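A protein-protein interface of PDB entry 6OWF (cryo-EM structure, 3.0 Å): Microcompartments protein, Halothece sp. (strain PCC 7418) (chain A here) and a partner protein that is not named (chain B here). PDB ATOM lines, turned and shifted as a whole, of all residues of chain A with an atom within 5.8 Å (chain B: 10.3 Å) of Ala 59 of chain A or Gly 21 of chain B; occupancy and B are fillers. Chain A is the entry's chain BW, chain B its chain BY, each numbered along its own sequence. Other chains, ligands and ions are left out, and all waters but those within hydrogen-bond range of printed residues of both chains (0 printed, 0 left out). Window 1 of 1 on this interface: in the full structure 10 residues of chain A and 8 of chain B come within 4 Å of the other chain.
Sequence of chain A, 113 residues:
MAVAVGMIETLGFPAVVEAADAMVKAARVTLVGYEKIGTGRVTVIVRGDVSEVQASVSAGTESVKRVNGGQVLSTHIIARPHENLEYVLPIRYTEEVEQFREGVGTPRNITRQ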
ATOM      1  N   ALA A  22       3.493  -1.099   7.044  1.00  0.00           N
ATOM      2  CA  ALA A  22       2.373  -0.436   6.391  1.00  0.00           C
ATOM      3  C   ALA A  22       1.068  -1.181   6.619  1.00  0.00           C
ATOM      4  O   ALA A  22       0.003  -0.682   6.251  1.00  0.00           O
ATOM      5  CB  ALA A  22       2.641  -0.285   4.898  1.00  0.00           C
ATOM      6  N   MET A  23       1.127  -2.384   7.190  1.00  0.00           N
ATOM      7  CA  MET A  23      -0.092  -3.058   7.614  1.00  0.00           C
ATOM      8  C   MET A  23      -0.568  -2.531   8.960  1.00  0.00           C
ATOM      9  O   MET A  23      -1.746  -2.204   9.122  1.00  0.00           O
ATOM     10  CB  MET A  23       0.135  -4.566   7.669  1.00  0.00           C
ATOM     11  CG  MET A  23      -0.128  -5.268   6.354  1.00  0.00           C
ATOM     12  SD  MET A  23      -0.596  -6.992   6.531  1.00  0.00           S
ATOM     13  CE  MET A  23       1.008  -7.748   6.695  1.00  0.00           C
ATOM     14  N   ALA A  26      -1.836   1.118   8.548  1.00  0.00           N
ATOM     15  CA  ALA A  26      -3.019   1.389   7.738  1.00  0.00           C
ATOM     16  C   ALA A  26      -4.298   1.188   8.536  1.00  0.00           C
ATOM     17  O   ALA A  26      -5.280   1.913   8.342  1.00  0.00           O
ATOM     18  CB  ALA A  26      -3.031   0.501   6.497  1.00  0.00           C
ATOM     19  N   GLN A  54      -8.574  -6.513   6.105  1.00  0.00           N
ATOM     20  CA  GLN A  54      -8.745  -6.358   4.663  1.00  0.00           C
ATOM     21  C   GLN A  54      -8.138  -5.054   4.170  1.00  0.00           C
ATOM     22  O   GLN A  54      -7.586  -4.996   3.069  1.00  0.00           O
ATOM     23  CB  GLN A  54     -10.223  -6.401   4.290  1.00  0.00           C
ATOM     24  CG  GLN A  54     -10.832  -7.776   4.212  1.00  0.00           C
ATOM     25  CD  GLN A  54     -12.221  -7.736   3.620  1.00  0.00           C
ATOM     26  OE1 GLN A  54     -12.440  -7.137   2.568  1.00  0.00           O
ATOM     27  NE2 GLN A  54     -13.175  -8.347   4.306  1.00  0.00           N
ATOM     28  N   ALA A  55      -8.231  -3.999   4.978  1.00  0.00           N
ATOM     29  CA  ALA A  55      -7.660  -2.717   4.586  1.00  0.00           C
ATOM     30  C   ALA A  55      -6.146  -2.731   4.707  1.00  0.00           C
ATOM     31  O   ALA A  55      -5.449  -2.151   3.870  1.00  0.00           O
ATOM     32  CB  ALA A  55      -8.253  -1.597   5.437  1.00  0.00           C
ATOM     33  N   SER A  56      -5.620  -3.394   5.737  1.00  0.00           N
ATOM     34  CA  SER A  56      -4.182  -3.394   5.976  1.00  0.00           C
ATOM     35  C   SER A  56      -3.444  -4.251   4.958  1.00  0.00           C
ATOM     36  O   SER A  56      -2.395  -3.846   4.447  1.00  0.00           O
ATOM     37  CB  SER A  56      -3.894  -3.889   7.387  1.00  0.00           C
ATOM     38  OG  SER A  56      -4.256  -5.246   7.531  1.00  0.00           O
ATOM     39  N   VAL A  57      -3.974  -5.441   4.662  1.00  0.00           N
ATOM     40  CA  VAL A  57      -3.346  -6.342   3.699  1.00  0.00           C
ATOM     41  C   VAL A  57      -3.384  -5.742   2.297  1.00  0.00           C
ATOM     42  O   VAL A  57      -2.415  -5.851   1.532  1.00  0.00           O
ATOM     43  CB  VAL A  57      -4.029  -7.723   3.771  1.00  0.00           C
ATOM     44  CG1 VAL A  57      -3.674  -8.595   2.594  1.00  0.00           C
ATOM     45  CG2 VAL A  57      -3.648  -8.426   5.054  1.00  0.00           C
ATOM     46  N   SER A  58      -4.475  -5.047   1.959  1.00  0.00           N
ATOM     47  CA  SER A  58      -4.557  -4.388   0.660  1.00  0.00           C
ATOM     48  C   SER A  58      -3.618  -3.190   0.590  1.00  0.00           C
ATOM     49  O   SER A  58      -3.005  -2.931  -0.446  1.00  0.00           O
ATOM     50  CB  SER A  58      -5.993  -3.967   0.375  1.00  0.00           C
ATOM     51  OG  SER A  58      -6.841  -5.096   0.263  1.00  0.00           O
ATOM     52  N   ALA A  59      -3.477  -2.455   1.694  1.00  0.00           N
ATOM     53  CA  ALA A  59      -2.555  -1.322   1.713  1.00  0.00           C
ATOM     54  C   ALA A  59      -1.119  -1.782   1.889  1.00  0.00           C
ATOM     55  O   ALA A  59      -0.184  -1.088   1.475  1.00  0.00           O
ATOM     56  CB  ALA A  59      -2.932  -0.339   2.819  1.00  0.00           C
ATOM     57  N   GLY A  60      -0.924  -2.941   2.515  1.00  0.00           N
ATOM     58  CA  GLY A  60       0.418  -3.474   2.655  1.00  0.00           C
ATOM     59  C   GLY A  60       0.949  -4.070   1.365  1.00  0.00           C
ATOM     60  O   GLY A  60       2.152  -4.294   1.227  1.00  0.00           O
ATOM     61  N   THR A  61       0.062  -4.344   0.407  1.00  0.00           N
ATOM     62  CA  THR A  61       0.486  -4.966  -0.841  1.00  0.00           C
ATOM     63  C   THR A  61       1.143  -3.977  -1.796  1.00  0.00           C
ATOM     64  O   THR A  61       2.165  -4.314  -2.404  1.00  0.00           O
ATOM     65  CB  THR A  61      -0.707  -5.646  -1.513  1.00  0.00           C
ATOM     66  OG1 THR A  61      -1.420  -6.423  -0.545  1.00  0.00           O
ATOM     67  CG2 THR A  61      -0.254  -6.561  -2.637  1.00  0.00           C
ATOM     68  N   GLU A  62       0.601  -2.766  -1.944  1.00  0.00           N
ATOM     69  CA  GLU A  62       1.241  -1.761  -2.788  1.00  0.00           C
ATOM     70  C   GLU A  62       2.330  -0.976  -2.076  1.00  0.00           C
ATOM     71  O   GLU A  62       2.854  -0.017  -2.653  1.00  0.00           O
ATOM     72  CB  GLU A  62       0.222  -0.774  -3.372  1.00  0.00           C
ATOM     73  CG  GLU A  62      -0.683  -1.369  -4.436  1.00  0.00           C
ATOM     74  CD  GLU A  62      -2.016  -1.789  -3.887  1.00  0.00           C
ATOM     75  OE1 GLU A  62      -2.297  -1.435  -2.730  1.00  0.00           O
ATOM     76  OE2 GLU A  62      -2.780  -2.466  -4.605  1.00  0.00           O
ATOM     77  N   SER A  63       2.675  -1.337  -0.843  1.00  0.00           N
ATOM     78  CA  SER A  63       3.823  -0.717  -0.196  1.00  0.00           C
ATOM     79  C   SER A  63       5.097  -1.477  -0.535  1.00  0.00           C
ATOM     80  O   SER A  63       6.190  -0.905  -0.563  1.00  0.00           O
ATOM     81  CB  SER A  63       3.601  -0.662   1.311  1.00  0.00           C
ATOM     82  OG  SER A  63       2.378  -0.015   1.606  1.00  0.00           O
ATOM     83  N   ARG A  66       6.668  -0.372  -3.819  1.00  0.00           N
ATOM     84  CA  ARG A  66       7.476   0.839  -3.838  1.00  0.00           C
ATOM     85  C   ARG A  66       8.822   0.582  -3.176  1.00  0.00           C
ATOM     86  O   ARG A  66       9.503   1.517  -2.745  1.00  0.00           O
ATOM     87  CB  ARG A  66       6.740   1.986  -3.147  1.00  0.00           C
ATOM     88  CG  ARG A  66       5.322   2.186  -3.647  1.00  0.00           C
ATOM     89  CD  ARG A  66       4.676   3.394  -3.005  1.00  0.00           C
ATOM     90  NE  ARG A  66       3.227   3.253  -2.933  1.00  0.00           N
ATOM     91  CZ  ARG A  66       2.541   3.169  -1.801  1.00  0.00           C
ATOM     92  NH1 ARG A  66       3.172   3.213  -0.635  1.00  0.00           N
ATOM     93  NH2 ARG A  66       1.223   3.043  -1.831  1.00  0.00           N
ATOM     94  N   THR B   9      -6.401   6.932  11.436  1.00  0.00           N
ATOM     95  CA  THR B   9      -6.616   6.293  10.150  1.00  0.00           C
ATOM     96  C   THR B   9      -8.107   6.083   9.916  1.00  0.00           C
ATOM     97  O   THR B   9      -8.892   6.018  10.865  1.00  0.00           O
ATOM     98  CB  THR B   9      -5.858   4.961  10.068  1.00  0.00           C
ATOM     99  OG1 THR B   9      -6.073   4.357   8.788  1.00  0.00           O
ATOM    100  CG2 THR B   9      -6.301   4.006  11.161  1.00  0.00           C
ATOM    101  N   VAL B  10      -8.494   6.013   8.646  1.00  0.00           N
ATOM    102  CA  VAL B  10      -9.881   5.823   8.236  1.00  0.00           C
ATOM    103  C   VAL B  10      -9.939   4.595   7.338  1.00  0.00           C
ATOM    104  O   VAL B  10      -9.176   4.490   6.372  1.00  0.00           O
ATOM    105  CB  VAL B  10     -10.431   7.064   7.512  1.00  0.00           C
ATOM    106  CG1 VAL B  10     -11.824   6.805   6.976  1.00  0.00           C
ATOM    107  CG2 VAL B  10     -10.447   8.262   8.439  1.00  0.00           C
ATOM    108  N   VAL B  11     -10.835   3.667   7.659  1.00  0.00           N
ATOM    109  CA  VAL B  11     -10.996   2.427   6.912  1.00  0.00           C
ATOM    110  C   VAL B  11     -12.378   2.430   6.281  1.00  0.00           C
ATOM    111  O   VAL B  11     -13.385   2.586   6.981  1.00  0.00           O
ATOM    112  CB  VAL B  11     -10.804   1.196   7.816  1.00  0.00           C
ATOM    113  CG1 VAL B  11     -11.301  -0.057   7.134  1.00  0.00           C
ATOM    114  CG2 VAL B  11      -9.346   1.050   8.198  1.00  0.00           C
ATOM    115  N   GLY B  12     -12.426   2.280   4.962  1.00  0.00           N
ATOM    116  CA  GLY B  12     -13.687   2.169   4.260  1.00  0.00           C
ATOM    117  C   GLY B  12     -13.765   0.890   3.459  1.00  0.00           C
ATOM    118  O   GLY B  12     -12.906   0.635   2.613  1.00  0.00           O
ATOM    119  N   THR B  13     -14.782   0.070   3.719  1.00  0.00           N
ATOM    120  CA  THR B  13     -14.880  -1.210   3.029  1.00  0.00           C
ATOM    121  C   THR B  13     -15.633  -1.082   1.713  1.00  0.00           C
ATOM    122  O   THR B  13     -15.171  -1.578   0.680  1.00  0.00           O
ATOM    123  CB  THR B  13     -15.553  -2.244   3.930  1.00  0.00           C
ATOM    124  OG1 THR B  13     -14.997  -2.157   5.245  1.00  0.00           O
ATOM    125  CG2 THR B  13     -15.321  -3.642   3.393  1.00  0.00           C
ATOM    126  N   LYS B  15     -16.306   0.935  -1.248  1.00  0.00           N
ATOM    127  CA  LYS B  15     -15.648   2.059  -1.896  1.00  0.00           C
ATOM    128  C   LYS B  15     -15.544   1.777  -3.384  1.00  0.00           C
ATOM    129  O   LYS B  15     -15.988   0.737  -3.873  1.00  0.00           O
ATOM    130  CB  LYS B  15     -14.268   2.315  -1.294  1.00  0.00           C
ATOM    131  CG  LYS B  15     -13.357   1.111  -1.312  1.00  0.00           C
ATOM    132  CD  LYS B  15     -12.069   1.401  -0.573  1.00  0.00           C
ATOM    133  CE  LYS B  15     -11.319   0.127  -0.261  1.00  0.00           C
ATOM    134  NZ  LYS B  15     -10.255   0.367   0.749  1.00  0.00           N
ATOM    135  N   LEU B  16     -14.961   2.731  -4.099  1.00  0.00           N
ATOM    136  CA  LEU B  16     -14.734   2.569  -5.523  1.00  0.00           C
ATOM    137  C   LEU B  16     -13.641   1.527  -5.758  1.00  0.00           C
ATOM    138  O   LEU B  16     -12.790   1.308  -4.891  1.00  0.00           O
ATOM    139  CB  LEU B  16     -14.338   3.907  -6.144  1.00  0.00           C
ATOM    140  CG  LEU B  16     -15.416   4.988  -6.154  1.00  0.00           C
ATOM    141  CD1 LEU B  16     -14.909   6.225  -6.850  1.00  0.00           C
ATOM    142  CD2 LEU B  16     -16.670   4.482  -6.832  1.00  0.00           C
ATOM    143  N   PRO B  17     -13.650   0.850  -6.911  1.00  0.00           N
ATOM    144  CA  PRO B  17     -12.554  -0.089  -7.205  1.00  0.00           C
ATOM    145  C   PRO B  17     -11.222   0.596  -7.448  1.00  0.00           C
ATOM    146  O   PRO B  17     -10.171  -0.044  -7.323  1.00  0.00           O
ATOM    147  CB  PRO B  17     -13.046  -0.820  -8.462  1.00  0.00           C
ATOM    148  CG  PRO B  17     -14.515  -0.602  -8.489  1.00  0.00           C
ATOM    149  CD  PRO B  17     -14.733   0.748  -7.902  1.00  0.00           C
ATOM    150  N   SER B  18     -11.235   1.883  -7.800  1.00  0.00           N
ATOM    151  CA  SER B  18      -9.993   2.633  -7.928  1.00  0.00           C
ATOM    152  C   SER B  18      -9.398   2.960  -6.566  1.00  0.00           C
ATOM    153  O   SER B  18      -8.196   3.224  -6.464  1.00  0.00           O
ATOM    154  CB  SER B  18     -10.241   3.914  -8.717  1.00  0.00           C
ATOM    155  OG  SER B  18     -10.682   3.624 -10.030  1.00  0.00           O
ATOM    156  N   MET B  19     -10.218   2.951  -5.517  1.00  0.00           N
ATOM    157  CA  MET B  19      -9.761   3.316  -4.184  1.00  0.00           C
ATOM    158  C   MET B  19      -9.241   2.132  -3.384  1.00  0.00           C
ATOM    159  O   MET B  19      -8.984   2.288  -2.186  1.00  0.00           O
ATOM    160  CB  MET B  19     -10.896   3.986  -3.414  1.00  0.00           C
ATOM    161  CG  MET B  19     -11.235   5.368  -3.913  1.00  0.00           C
ATOM    162  SD  MET B  19     -10.031   6.581  -3.363  1.00  0.00           S
ATOM    163  CE  MET B  19     -10.433   6.661  -1.622  1.00  0.00           C
ATOM    164  N   THR B  20      -9.088   0.963  -3.997  1.00  0.00           N
ATOM    165  CA  THR B  20      -8.609  -0.198  -3.262  1.00  0.00           C
ATOM    166  C   THR B  20      -7.101  -0.127  -3.081  1.00  0.00           C
ATOM    167  O   THR B  20      -6.365   0.250  -3.997  1.00  0.00           O
ATOM    168  CB  THR B  20      -8.986  -1.491  -3.982  1.00  0.00           C
ATOM    169  OG1 THR B  20      -8.608  -1.399  -5.360  1.00  0.00           O
ATOM    170  CG2 THR B  20     -10.481  -1.737  -3.885  1.00  0.00           C
ATOM    171  N   GLY B  21      -6.642  -0.489  -1.888  1.00  0.00           N
ATOM    172  CA  GLY B  21      -5.232  -0.458  -1.579  1.00  0.00           C
ATOM    173  C   GLY B  21      -4.677   0.905  -1.236  1.00  0.00           C
ATOM    174  O   GLY B  21      -3.460   1.033  -1.065  1.00  0.00           O
ATOM    175  N   VAL B  22      -5.522   1.922  -1.132  1.00  0.00           N
ATOM    176  CA  VAL B  22      -5.093   3.275  -0.812  1.00  0.00           C
ATOM    177  C   VAL B  22      -5.246   3.469   0.687  1.00  0.00           C
ATOM    178  O   VAL B  22      -6.350   3.352   1.229  1.00  0.00           O
ATOM    179  CB  VAL B  22      -5.899   4.320  -1.598  1.00  0.00           C
ATOM    180  CG1 VAL B  22      -5.631   5.708  -1.061  1.00  0.00           C
ATOM    181  CG2 VAL B  22      -5.545   4.246  -3.063  1.00  0.00           C
ATOM    182  N   LYS B  23      -4.136   3.753   1.356  1.00  0.00           N
ATOM    183  CA  LYS B  23      -4.129   3.944   2.798  1.00  0.00           C
ATOM    184  C   LYS B  23      -4.623   5.348   3.117  1.00  0.00           C
ATOM    185  O   LYS B  23      -3.987   6.336   2.737  1.00  0.00           O
ATOM    186  CB  LYS B  23      -2.722   3.709   3.335  1.00  0.00           C
ATOM    187  CG  LYS B  23      -2.460   4.195   4.736  1.00  0.00           C
ATOM    188  CD  LYS B  23      -0.989   4.016   5.057  1.00  0.00           C
ATOM    189  CE  LYS B  23      -0.641   4.536   6.434  1.00  0.00           C
ATOM    190  NZ  LYS B  23       0.813   4.396   6.705  1.00  0.00           N
ATOM    191  N   LEU B  24      -5.760   5.440   3.797  1.00  0.00           N
ATOM    192  CA  LEU B  24      -6.401   6.712   4.100  1.00  0.00           C
ATOM    193  C   LEU B  24      -6.130   7.089   5.547  1.00  0.00           C
ATOM    194  O   LEU B  24      -6.577   6.398   6.465  1.00  0.00           O
ATOM    195  CB  LEU B  24      -7.907   6.639   3.852  1.00  0.00           C
ATOM    196  CG  LEU B  24      -8.330   6.204   2.452  1.00  0.00           C
ATOM    197  CD1 LEU B  24      -9.641   5.448   2.506  1.00  0.00           C
ATOM    198  CD2 LEU B  24      -8.439   7.407   1.542  1.00  0.00           C
ATOM    199  N   LEU B  25      -5.413   8.186   5.742  1.00  0.00           N
ATOM    200  CA  LEU B  25      -5.075   8.686   7.063  1.00  0.00           C
ATOM    201  C   LEU B  25      -6.126   9.674   7.537  1.00  0.00           C
ATOM    202  O   LEU B  25      -7.088   9.981   6.836  1.00  0.00           O
ATOM    203  CB  LEU B  25      -3.703   9.359   7.055  1.00  0.00           C
ATOM    204  CG  LEU B  25      -2.502   8.444   6.895  1.00  0.00           C
ATOM    205  CD1 LEU B  25      -1.255   9.276   7.007  1.00  0.00           C
ATOM    206  CD2 LEU B  25      -2.531   7.367   7.957  1.00  0.00           C
ATOM    207  N   ALA B  43      -6.352  11.906   3.906  1.00  0.00           N
ATOM    208  CA  ALA B  43      -5.405  11.956   2.806  1.00  0.00           C
ATOM    209  C   ALA B  43      -4.826  10.580   2.530  1.00  0.00           C
ATOM    210  O   ALA B  43      -4.659   9.764   3.438  1.00  0.00           O
ATOM    211  CB  ALA B  43      -4.271  12.933   3.101  1.00  0.00           C
ATOM    212  N   ALA B  44      -4.519  10.336   1.259  1.00  0.00           N
ATOM    213  CA  ALA B  44      -3.770   9.151   0.875  1.00  0.00           C
ATOM    214  C   ALA B  44      -2.340   9.249   1.385  1.00  0.00           C
ATOM    215  O   ALA B  44      -1.839  10.333   1.692  1.00  0.00           O
ATOM    216  CB  ALA B  44      -3.774   8.985  -0.641  1.00  0.00           C
ATOM    217  N   ASP B  45      -1.671   8.106   1.468  1.00  0.00           N
ATOM    218  CA  ASP B  45      -0.377   8.009   2.138  1.00  0.00           C
ATOM    219  C   ASP B  45       0.514   7.013   1.408  1.00  0.00           C
ATOM    220  O   ASP B  45       0.503   5.813   1.705  1.00  0.00           O
ATOM    221  CB  ASP B  45      -0.576   7.628   3.604  1.00  0.00           C
ATOM    222  CG  ASP B  45       0.717   7.522   4.359  1.00  0.00           C
ATOM    223  OD1 ASP B  45       1.153   8.542   4.923  1.00  0.00           O
ATOM    224  OD2 ASP B  45       1.287   6.413   4.418  1.00  0.00           O
ATOM    225  N   PRO B  46       1.285   7.476   0.420  1.00  0.00           N
ATOM    226  CA  PRO B  46       2.263   6.578  -0.208  1.00  0.00           C
ATOM    227  C   PRO B  46       3.482   6.332   0.658  1.00  0.00           C
ATOM    228  O   PRO B  46       3.928   5.186   0.776  1.00  0.00           O
ATOM    229  CB  PRO B  46       2.626   7.309  -1.509  1.00  0.00           C
ATOM    230  CG  PRO B  46       1.650   8.434  -1.629  1.00  0.00           C
ATOM    231  CD  PRO B  46       1.243   8.780  -0.248  1.00  0.00           C
ATOM    232  N   VAL B  47       4.037   7.375   1.268  1.00  0.00           N
ATOM    233  CA  VAL B  47       5.148   7.243   2.200  1.00  0.00           C
ATOM    234  C   VAL B  47       4.575   7.004   3.591  1.00  0.00           C
ATOM    235  O   VAL B  47       3.788   7.811   4.096  1.00  0.00           O
ATOM    236  CB  VAL B  47       6.081   8.467   2.153  1.00  0.00           C
ATOM    237  CG1 VAL B  47       6.945   8.395   0.919  1.00  0.00           C
ATOM    238  CG2 VAL B  47       5.295   9.772   2.089  1.00  0.00           C
ATOM    239  N   GLY B  48       4.955   5.884   4.202  1.00  0.00           N
ATOM    240  CA  GLY B  48       4.331   5.414   5.426  1.00  0.00           C
ATOM    241  C   GLY B  48       4.488   6.316   6.632  1.00  0.00           C
ATOM    242  O   GLY B  48       5.579   6.435   7.194  1.00  0.00           O
ATOM    243  N   TYR B  68       0.968   5.995  -9.547  1.00  0.00           N
ATOM    244  CA  TYR B  68       0.072   4.974  -9.032  1.00  0.00           C
ATOM    245  C   TYR B  68      -1.198   5.561  -8.446  1.00  0.00           C
ATOM    246  O   TYR B  68      -2.104   4.801  -8.086  1.00  0.00           O
ATOM    247  CB  TYR B  68       0.766   4.106  -7.970  1.00  0.00           C
ATOM    248  CG  TYR B  68       1.745   4.835  -7.084  1.00  0.00           C
ATOM    249  CD1 TYR B  68       1.304   5.600  -6.012  1.00  0.00           C
ATOM    250  CD2 TYR B  68       3.112   4.743  -7.308  1.00  0.00           C
ATOM    251  CE1 TYR B  68       2.199   6.262  -5.192  1.00  0.00           C
ATOM    252  CE2 TYR B  68       4.015   5.404  -6.496  1.00  0.00           C
ATOM    253  CZ  TYR B  68       3.551   6.161  -5.440  1.00  0.00           C
ATOM    254  OH  TYR B  68       4.446   6.818  -4.631  1.00  0.00           O
ATOM    255  N   HIS B  69      -1.288   6.885  -8.342  1.00  0.00           N
ATOM    256  CA  HIS B  69      -2.501   7.579  -7.947  1.00  0.00           C
ATOM    257  C   HIS B  69      -3.121   8.347  -9.105  1.00  0.00           C
ATOM    258  O   HIS B  69      -3.933   9.245  -8.872  1.00  0.00           O
ATOM    259  CB  HIS B  69      -2.207   8.535  -6.792  1.00  0.00           C
ATOM    260  CG  HIS B  69      -1.919   7.850  -5.493  1.00  0.00           C
ATOM    261  ND1 HIS B  69      -1.598   8.542  -4.346  1.00  0.00           N
ATOM    262  CD2 HIS B  69      -1.920   6.541  -5.153  1.00  0.00           C
ATOM    263  CE1 HIS B  69      -1.408   7.687  -3.357  1.00  0.00           C
ATOM    264  NE2 HIS B  69      -1.596   6.466  -3.821  1.00  0.00           N
ATOM    265  N   ARG B  72      -6.986   7.609  -9.919  1.00  0.00           N
ATOM    266  CA  ARG B  72      -7.674   7.421  -8.658  1.00  0.00           C
ATOM    267  C   ARG B  72      -8.366   8.709  -8.230  1.00  0.00           C
ATOM    268  O   ARG B  72      -7.873   9.805  -8.502  1.00  0.00           O
ATOM    269  CB  ARG B  72      -6.692   6.984  -7.568  1.00  0.00           C
ATOM    270  CG  ARG B  72      -6.023   5.656  -7.844  1.00  0.00           C
ATOM    271  CD  ARG B  72      -5.215   5.202  -6.651  1.00  0.00           C
ATOM    272  NE  ARG B  72      -4.343   4.081  -6.981  1.00  0.00           N
ATOM    273  CZ  ARG B  72      -4.662   2.806  -6.795  1.00  0.00           C
ATOM    274  NH1 ARG B  72      -3.805   1.850  -7.124  1.00  0.00           N
ATOM    275  NH2 ARG B  72      -5.839   2.485  -6.279  1.00  0.00           N
ATOM    276  N   LEU B  74      -8.471  10.927  -5.859  1.00  0.00           N
ATOM    277  CA  LEU B  74      -7.786  11.439  -4.681  1.00  0.00           C
ATOM    278  C   LEU B  74      -7.606  12.943  -4.798  1.00  0.00           C
ATOM    279  O   LEU B  74      -7.134  13.438  -5.825  1.00  0.00           O
ATOM    280  CB  LEU B  74      -6.425  10.771  -4.504  1.00  0.00           C
ATOM    281  CG  LEU B  74      -6.454   9.264  -4.298  1.00  0.00           C
ATOM    282  CD1 LEU B  74      -5.050   8.756  -4.202  1.00  0.00           C
ATOM    283  CD2 LEU B  74      -7.216   8.930  -3.043  1.00  0.00           C
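Val 11 of chain B touches Ala 55 of chain A. Ser 58 of chain A touches Gly 21 of chain B (O to CA, 3.5 Å). Ala 59 of chain A touches Gly 21 of chain B (CA to O, 3.8 Å). Arg 66 of chain A touches Tyr 68 of chain B (CD to OH, 3.8 Å).
The backbone carbonyl oxygen of Gln 54 of chain A sits at hydrogen-bond distance from the side-chain hydroxyl of Ser 58 of chain A (2.9 Å). O of Ala 59 of chain A lies within hydrogen-bond range of OG of Ser 63 of chain A, at 2.8 Å. NE of Arg 66 of chain A sits at hydrogen-bond distance from O of Glu 62 of chain A (3.3 Å). The side-chain hydroxyl (OG1) of Thr 9 of chain B lies within hydrogen-bond range of the backbone carbonyl oxygen (O) of Leu 24 of chain B. The backbone carbonyl oxygen of Tyr 68 of chain B lies within hydrogen-bond range of the guanidinium group of Arg 72 of chain B, 2.6 Å away.
Ala 59 of chain A touches one residue of chain B. Gly 21 of chain B touches three residues of chain A. Ser 58 of chain A touches just one residue of chain B: Gly 21. No residue of chain B comes within 4 Å of Gly 60 of chain A. Of the printed residues of chain B, Arg 66 of chain A touches Pro 46 (2.5 Å) and Tyr 68 (3.8 Å). Printed residues of chain A within 4 Å of Thr 9 of chain B: Ala 26 (2.6 Å). The nearest residue of chain A that does not touch Gly 21 of chain B is Arg 66 of chain A (5.2 Å).
O of Ala 26 of chain A is in hydrogen-bond range of OG1 of Thr 9 of chain B (2.6 Å). O of Pro 46 of chain B sits at hydrogen-bond distance from NH1 of Arg 66 of chain A (2.5 Å). OE1 of Glu 62 of chain A lies close to O of Gly 21 of chain B (3.2 Å).
Printed residues of chain B that touch a printed residue of chain A: Thr 9, Val 11, Gly 21, Pro 46 and Tyr 68. Hydrophobic or aromatic side chains of chain B that line the printed part of chain A: Val 11 and Tyr 68. Of the 14 printed residues of chain A, 6 touch a printed residue of chain B.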
